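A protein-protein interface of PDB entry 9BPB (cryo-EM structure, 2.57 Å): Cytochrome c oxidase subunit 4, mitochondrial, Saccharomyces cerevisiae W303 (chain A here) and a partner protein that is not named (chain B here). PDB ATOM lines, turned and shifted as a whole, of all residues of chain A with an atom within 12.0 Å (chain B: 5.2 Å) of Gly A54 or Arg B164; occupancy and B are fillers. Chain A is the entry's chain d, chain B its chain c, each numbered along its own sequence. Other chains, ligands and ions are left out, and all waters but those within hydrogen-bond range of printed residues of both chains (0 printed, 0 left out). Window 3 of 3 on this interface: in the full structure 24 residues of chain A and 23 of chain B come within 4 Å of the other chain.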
ATOM      1  N   GLY A  50      -3.148 -39.407 -12.584  1.00  0.00           N
ATOM      2  CA  GLY A  50      -3.162 -38.227 -11.747  1.00  0.00           C
ATOM      3  C   GLY A  50      -2.100 -37.220 -12.138  1.00  0.00           C
ATOM      4  O   GLY A  50      -1.144 -37.516 -12.855  1.00  0.00           O
ATOM      5  N   ALA A  51      -2.282 -35.996 -11.654  1.00  0.00           N
ATOM      6  CA  ALA A  51      -1.332 -34.932 -11.938  1.00  0.00           C
ATOM      7  C   ALA A  51      -0.025 -35.163 -11.191  1.00  0.00           C
ATOM      8  O   ALA A  51      -0.019 -35.587 -10.032  1.00  0.00           O
ATOM      9  CB  ALA A  51      -1.918 -33.577 -11.554  1.00  0.00           C
ATOM     10  N   LYS A  52       1.084 -34.878 -11.862  1.00  0.00           N
ATOM     11  CA  LYS A  52       2.389 -34.992 -11.235  1.00  0.00           C
ATOM     12  C   LYS A  52       2.582 -33.879 -10.209  1.00  0.00           C
ATOM     13  O   LYS A  52       1.988 -32.801 -10.300  1.00  0.00           O
ATOM     14  CB  LYS A  52       3.492 -34.943 -12.292  1.00  0.00           C
ATOM     15  CG  LYS A  52       3.438 -36.101 -13.269  1.00  0.00           C
ATOM     16  CD  LYS A  52       4.564 -36.038 -14.283  1.00  0.00           C
ATOM     17  CE  LYS A  52       4.442 -37.167 -15.294  1.00  0.00           C
ATOM     18  NZ  LYS A  52       4.635 -38.497 -14.655  1.00  0.00           N
ATOM     19  N   GLU A  53       3.421 -34.158  -9.214  1.00  0.00           N
ATOM     20  CA  GLU A  53       3.640 -33.204  -8.136  1.00  0.00           C
ATOM     21  C   GLU A  53       4.286 -31.931  -8.666  1.00  0.00           C
ATOM     22  O   GLU A  53       5.215 -31.975  -9.477  1.00  0.00           O
ATOM     23  CB  GLU A  53       4.514 -33.827  -7.048  1.00  0.00           C
ATOM     24  CG  GLU A  53       4.048 -35.201  -6.592  1.00  0.00           C
ATOM     25  CD  GLU A  53       2.910 -35.129  -5.593  1.00  0.00           C
ATOM     26  OE1 GLU A  53       2.836 -34.129  -4.847  1.00  0.00           O
ATOM     27  OE2 GLU A  53       2.092 -36.071  -5.551  1.00  0.00           O
ATOM     28  N   GLY A  54       3.789 -30.789  -8.198  1.00  0.00           N
ATOM     29  CA  GLY A  54       4.294 -29.505  -8.637  1.00  0.00           C
ATOM     30  C   GLY A  54       3.644 -28.941  -9.879  1.00  0.00           C
ATOM     31  O   GLY A  54       4.138 -27.943 -10.415  1.00  0.00           O
ATOM     32  N   THR A  55       2.554 -29.540 -10.356  1.00  0.00           N
ATOM     33  CA  THR A  55       1.857 -29.073 -11.545  1.00  0.00           C
ATOM     34  C   THR A  55       0.373 -28.908 -11.246  1.00  0.00           C
ATOM     35  O   THR A  55      -0.168 -29.548 -10.343  1.00  0.00           O
ATOM     36  CB  THR A  55       2.036 -30.041 -12.722  1.00  0.00           C
ATOM     37  OG1 THR A  55       1.526 -31.330 -12.363  1.00  0.00           O
ATOM     38  CG2 THR A  55       3.504 -30.166 -13.096  1.00  0.00           C
ATOM     39  N   VAL A  56      -0.275 -28.040 -12.011  1.00  0.00           N
ATOM     40  CA  VAL A  56      -1.724 -27.859 -11.898  1.00  0.00           C
ATOM     41  C   VAL A  56      -2.419 -28.962 -12.692  1.00  0.00           C
ATOM     42  O   VAL A  56      -2.104 -29.152 -13.877  1.00  0.00           O
ATOM     43  CB  VAL A  56      -2.136 -26.478 -12.399  1.00  0.00           C
ATOM     44  CG1 VAL A  56      -3.629 -26.438 -12.668  1.00  0.00           C
ATOM     45  CG2 VAL A  56      -1.759 -25.416 -11.389  1.00  0.00           C
ATOM     46  N   PRO A  57      -3.345 -29.705 -12.088  1.00  0.00           N
ATOM     47  CA  PRO A  57      -3.990 -30.805 -12.813  1.00  0.00           C
ATOM     48  C   PRO A  57      -4.838 -30.301 -13.970  1.00  0.00           C
ATOM     49  O   PRO A  57      -5.406 -29.210 -13.920  1.00  0.00           O
ATOM     50  CB  PRO A  57      -4.858 -31.478 -11.741  1.00  0.00           C
ATOM     51  CG  PRO A  57      -4.317 -30.987 -10.432  1.00  0.00           C
ATOM     52  CD  PRO A  57      -3.828 -29.604 -10.704  1.00  0.00           C
ATOM     53  N   THR A  58      -4.914 -31.114 -15.019  1.00  0.00           N
ATOM     54  CA  THR A  58      -5.783 -30.837 -16.150  1.00  0.00           C
ATOM     55  C   THR A  58      -6.992 -31.769 -16.124  1.00  0.00           C
ATOM     56  O   THR A  58      -7.047 -32.738 -15.364  1.00  0.00           O
ATOM     57  CB  THR A  58      -5.021 -30.984 -17.469  1.00  0.00           C
ATOM     58  OG1 THR A  58      -4.276 -32.208 -17.458  1.00  0.00           O
ATOM     59  CG2 THR A  58      -4.067 -29.820 -17.668  1.00  0.00           C
ATOM     60  N   ASP A  61      -6.413 -35.273 -16.886  1.00  0.00           N
ATOM     61  CA  ASP A  61      -5.713 -36.003 -15.838  1.00  0.00           C
ATOM     62  C   ASP A  61      -6.675 -36.526 -14.777  1.00  0.00           C
ATOM     63  O   ASP A  61      -6.597 -37.693 -14.382  1.00  0.00           O
ATOM     64  CB  ASP A  61      -4.653 -35.110 -15.195  1.00  0.00           C
ATOM     65  CG  ASP A  61      -3.478 -34.846 -16.111  1.00  0.00           C
ATOM     66  OD1 ASP A  61      -3.209 -35.691 -16.989  1.00  0.00           O
ATOM     67  OD2 ASP A  61      -2.823 -33.795 -15.953  1.00  0.00           O
ATOM     68  N   GLN A  62      -7.594 -35.683 -14.306  1.00  0.00           N
ATOM     69  CA  GLN A  62      -8.376 -35.994 -13.117  1.00  0.00           C
ATOM     70  C   GLN A  62      -9.882 -35.885 -13.345  1.00  0.00           C
ATOM     71  O   GLN A  62     -10.600 -35.314 -12.523  1.00  0.00           O
ATOM     72  CB  GLN A  62      -7.948 -35.099 -11.955  1.00  0.00           C
ATOM     73  CG  GLN A  62      -6.914 -35.738 -11.049  1.00  0.00           C
ATOM     74  CD  GLN A  62      -6.239 -34.736 -10.137  1.00  0.00           C
ATOM     75  OE1 GLN A  62      -6.660 -33.584 -10.045  1.00  0.00           O
ATOM     76  NE2 GLN A  62      -5.183 -35.169  -9.463  1.00  0.00           N
ATOM     77  N   GLY B 162      -1.703 -22.408 -15.614  1.00  0.00           N
ATOM     78  CA  GLY B 162      -1.113 -23.710 -15.350  1.00  0.00           C
ATOM     79  C   GLY B 162      -0.003 -23.735 -14.319  1.00  0.00           C
ATOM     80  O   GLY B 162       0.581 -24.805 -14.104  1.00  0.00           O
ATOM     81  N   ASN B 163       0.336 -22.629 -13.662  1.00  0.00           N
ATOM     82  CA  ASN B 163       1.358 -22.635 -12.624  1.00  0.00           C
ATOM     83  C   ASN B 163       0.712 -22.534 -11.248  1.00  0.00           C
ATOM     84  O   ASN B 163      -0.156 -21.688 -11.014  1.00  0.00           O
ATOM     85  CB  ASN B 163       2.372 -21.505 -12.833  1.00  0.00           C
ATOM     86  CG  ASN B 163       1.742 -20.129 -12.803  1.00  0.00           C
ATOM     87  OD1 ASN B 163       0.526 -19.982 -12.905  1.00  0.00           O
ATOM     88  ND2 ASN B 163       2.576 -19.106 -12.658  1.00  0.00           N
ATOM     89  N   ARG B 164       1.134 -23.410 -10.337  1.00  0.00           N
ATOM     90  CA  ARG B 164       0.474 -23.536  -9.047  1.00  0.00           C
ATOM     91  C   ARG B 164       1.117 -22.703  -7.949  1.00  0.00           C
ATOM     92  O   ARG B 164       0.505 -22.537  -6.891  1.00  0.00           O
ATOM     93  CB  ARG B 164       0.433 -25.005  -8.608  1.00  0.00           C
ATOM     94  CG  ARG B 164       1.745 -25.559  -8.095  1.00  0.00           C
ATOM     95  CD  ARG B 164       1.657 -27.066  -7.924  1.00  0.00           C
ATOM     96  NE  ARG B 164       0.667 -27.464  -6.932  1.00  0.00           N
ATOM     97  CZ  ARG B 164       0.914 -27.606  -5.637  1.00  0.00           C
ATOM     98  NH1 ARG B 164       2.115 -27.378  -5.134  1.00  0.00           N
ATOM     99  NH2 ARG B 164      -0.069 -27.988  -4.827  1.00  0.00           N
ATOM    100  N   ASN B 165       2.325 -22.178  -8.160  1.00  0.00           N
ATOM    101  CA  ASN B 165       2.951 -21.376  -7.117  1.00  0.00           C
ATOM    102  C   ASN B 165       2.352 -19.979  -7.040  1.00  0.00           C
ATOM    103  O   ASN B 165       2.237 -19.417  -5.946  1.00  0.00           O
ATOM    104  CB  ASN B 165       4.459 -21.302  -7.339  1.00  0.00           C
ATOM    105  CG  ASN B 165       5.120 -22.662  -7.291  1.00  0.00           C
ATOM    106  OD1 ASN B 165       5.703 -23.115  -8.273  1.00  0.00           O
ATOM    107  ND2 ASN B 165       5.023 -23.325  -6.145  1.00  0.00           N
ATOM    108  N   LYS B 166       1.970 -19.398  -8.177  1.00  0.00           N
ATOM    109  CA  LYS B 166       1.270 -18.120  -8.164  1.00  0.00           C
ATOM    110  C   LYS B 166      -0.198 -18.262  -7.788  1.00  0.00           C
ATOM    111  O   LYS B 166      -0.743 -17.383  -7.111  1.00  0.00           O
ATOM    112  CB  LYS B 166       1.381 -17.435  -9.527  1.00  0.00           C
ATOM    113  CG  LYS B 166       2.730 -16.795  -9.793  1.00  0.00           C
ATOM    114  CD  LYS B 166       2.762 -16.134 -11.157  1.00  0.00           C
ATOM    115  CE  LYS B 166       1.836 -14.931 -11.207  1.00  0.00           C
ATOM    116  NZ  LYS B 166       1.948 -14.204 -12.500  1.00  0.00           N
ATOM    117  N   ALA B 167      -0.850 -19.342  -8.221  1.00  0.00           N
ATOM    118  CA  ALA B 167      -2.235 -19.584  -7.831  1.00  0.00           C
ATOM    119  C   ALA B 167      -2.347 -19.832  -6.333  1.00  0.00           C
ATOM    120  O   ALA B 167      -3.260 -19.320  -5.675  1.00  0.00           O
ATOM    121  CB  ALA B 167      -2.801 -20.764  -8.617  1.00  0.00           C
ATOM    122  N   LEU B 168      -1.423 -20.617  -5.776  1.00  0.00           N
ATOM    123  CA  LEU B 168      -1.466 -20.918  -4.351  1.00  0.00           C
ATOM    124  C   LEU B 168      -1.104 -19.696  -3.520  1.00  0.00           C
ATOM    125  O   LEU B 168      -1.614 -19.517  -2.409  1.00  0.00           O
ATOM    126  CB  LEU B 168      -0.527 -22.082  -4.040  1.00  0.00           C
ATOM    127  CG  LEU B 168      -0.919 -23.062  -2.938  1.00  0.00           C
ATOM    128  CD1 LEU B 168      -2.298 -23.628  -3.205  1.00  0.00           C
ATOM    129  CD2 LEU B 168       0.104 -24.179  -2.850  1.00  0.00           C
ATOM    130  N   SER B 169      -0.223 -18.842  -4.043  1.00  0.00           N
ATOM    131  CA  SER B 169       0.176 -17.649  -3.308  1.00  0.00           C
ATOM    132  C   SER B 169      -0.910 -16.582  -3.332  1.00  0.00           C
ATOM    133  O   SER B 169      -1.051 -15.823  -2.369  1.00  0.00           O
ATOM    134  CB  SER B 169       1.481 -17.093  -3.877  1.00  0.00           C
ATOM    135  OG  SER B 169       1.652 -15.731  -3.538  1.00  0.00           O
ATOM    136  N   MET B 230      -7.013 -26.857  -3.356  1.00  0.00           N
ATOM    137  CA  MET B 230      -5.934 -26.583  -4.341  1.00  0.00           C
ATOM    138  C   MET B 230      -4.622 -27.268  -3.930  1.00  0.00           C
ATOM    139  O   MET B 230      -3.968 -27.835  -4.817  1.00  0.00           O
ATOM    140  CB  MET B 230      -5.688 -25.083  -4.483  1.00  0.00           C
ATOM    141  CG  MET B 230      -4.715 -24.735  -5.589  1.00  0.00           C
ATOM    142  SD  MET B 230      -4.723 -22.975  -6.004  1.00  0.00           S
ATOM    143  CE  MET B 230      -6.482 -22.653  -6.080  1.00  0.00           C
ATOM    144  N   ARG B 231      -4.248 -27.228  -2.645  1.00  0.00           N
ATOM    145  CA  ARG B 231      -2.985 -27.822  -2.221  1.00  0.00           C
ATOM    146  C   ARG B 231      -2.981 -29.334  -2.404  1.00  0.00           C
ATOM    147  O   ARG B 231      -1.936 -29.914  -2.723  1.00  0.00           O
ATOM    148  CB  ARG B 231      -2.695 -27.469  -0.763  1.00  0.00           C
ATOM    149  CG  ARG B 231      -1.236 -27.622  -0.373  1.00  0.00           C
ATOM    150  CD  ARG B 231      -1.040 -27.526   1.131  1.00  0.00           C
ATOM    151  NE  ARG B 231      -1.498 -28.725   1.824  1.00  0.00           N
ATOM    152  CZ  ARG B 231      -0.704 -29.561   2.480  1.00  0.00           C
ATOM    153  NH1 ARG B 231       0.603 -29.367   2.541  1.00  0.00           N
ATOM    154  NH2 ARG B 231      -1.235 -30.618   3.087  1.00  0.00           N
ATOM    155  N   TYR B 233      -4.598 -31.015  -4.710  1.00  0.00           N
ATOM    156  CA  TYR B 233      -4.817 -31.390  -6.108  1.00  0.00           C
ATOM    157  C   TYR B 233      -6.273 -31.765  -6.381  1.00  0.00           C
ATOM    158  O   TYR B 233      -6.559 -32.711  -7.117  1.00  0.00           O
ATOM    159  CB  TYR B 233      -3.878 -32.523  -6.530  1.00  0.00           C
ATOM    160  CG  TYR B 233      -2.401 -32.194  -6.413  1.00  0.00           C
ATOM    161  CD1 TYR B 233      -1.781 -32.108  -5.171  1.00  0.00           C
ATOM    162  CD2 TYR B 233      -1.628 -31.978  -7.543  1.00  0.00           C
ATOM    163  CE1 TYR B 233      -0.439 -31.810  -5.061  1.00  0.00           C
ATOM    164  CE2 TYR B 233      -0.282 -31.679  -7.443  1.00  0.00           C
ATOM    165  CZ  TYR B 233       0.305 -31.596  -6.199  1.00  0.00           C
ATOM    166  OH  TYR B 233       1.643 -31.301  -6.088  1.00  0.00           O
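The backbone carbonyl oxygen of Tyr B233 sits close to the side-chain amide oxygen of Gln A62 (3.1 Å). OH of Tyr B233 lies within hydrogen-bond range of N of Gly A54, 3.1 Å away. OE1 of Glu A53 is in hydrogen-bond range of OH of Tyr B233 (3.3 Å).
The backbone carbonyl oxygen (O) of Arg B231 sits at hydrogen-bond distance from the guanidinium group (NH2) of Arg B164, 3.4 Å away. The backbone carbonyl oxygen (O) of Lys A52 lies within hydrogen-bond range of the side-chain hydroxyl (OG1) of Thr A55, 2.6 Å away.
Among the printed residues, pairs that only touch across the chains: Lys A52 with Tyr B233 (3.8 Å), Gly A54 with Arg B164 (3.4 Å), Thr A55 with Arg B164 (3.6 Å), Thr A55 with Tyr B233 (3.6 Å), Val A56 with Gly B162 (3.6 Å), Val A56 with Asn B163 (3.8 Å) and Val A56 with Arg B164 (3.6 Å).
Of chain B, only Arg B164 (3.4 Å) and Tyr B233 (3.1 Å) come within 4 Å of Gly A54. Of chain A, only Gly A54 (3.4 Å), Thr A55 (3.6 Å) and Val A56 (3.6 Å) come within 4 Å of Arg B164. Of chain A, only Val A56 comes within 4 Å of Asn B163. No residue of chain A comes within 4 Å of Ala B167. Printed residues of chain B within 4 Å of Thr A55: Arg B164 (3.6 Å) and Tyr B233 (3.6 Å). Of the printed residues of chain B, Glu A53 touches Tyr B233 (3.3 Å). Arg B231 touches none of the printed residues of chain A.
Hydrophobic or aromatic side chains of chain B that line the printed part of chain A: Tyr B233. Of the 11 printed residues of chain A, 6 touch a printed residue of chain B. Among the printed residues, 10 pairs touch across the chains.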
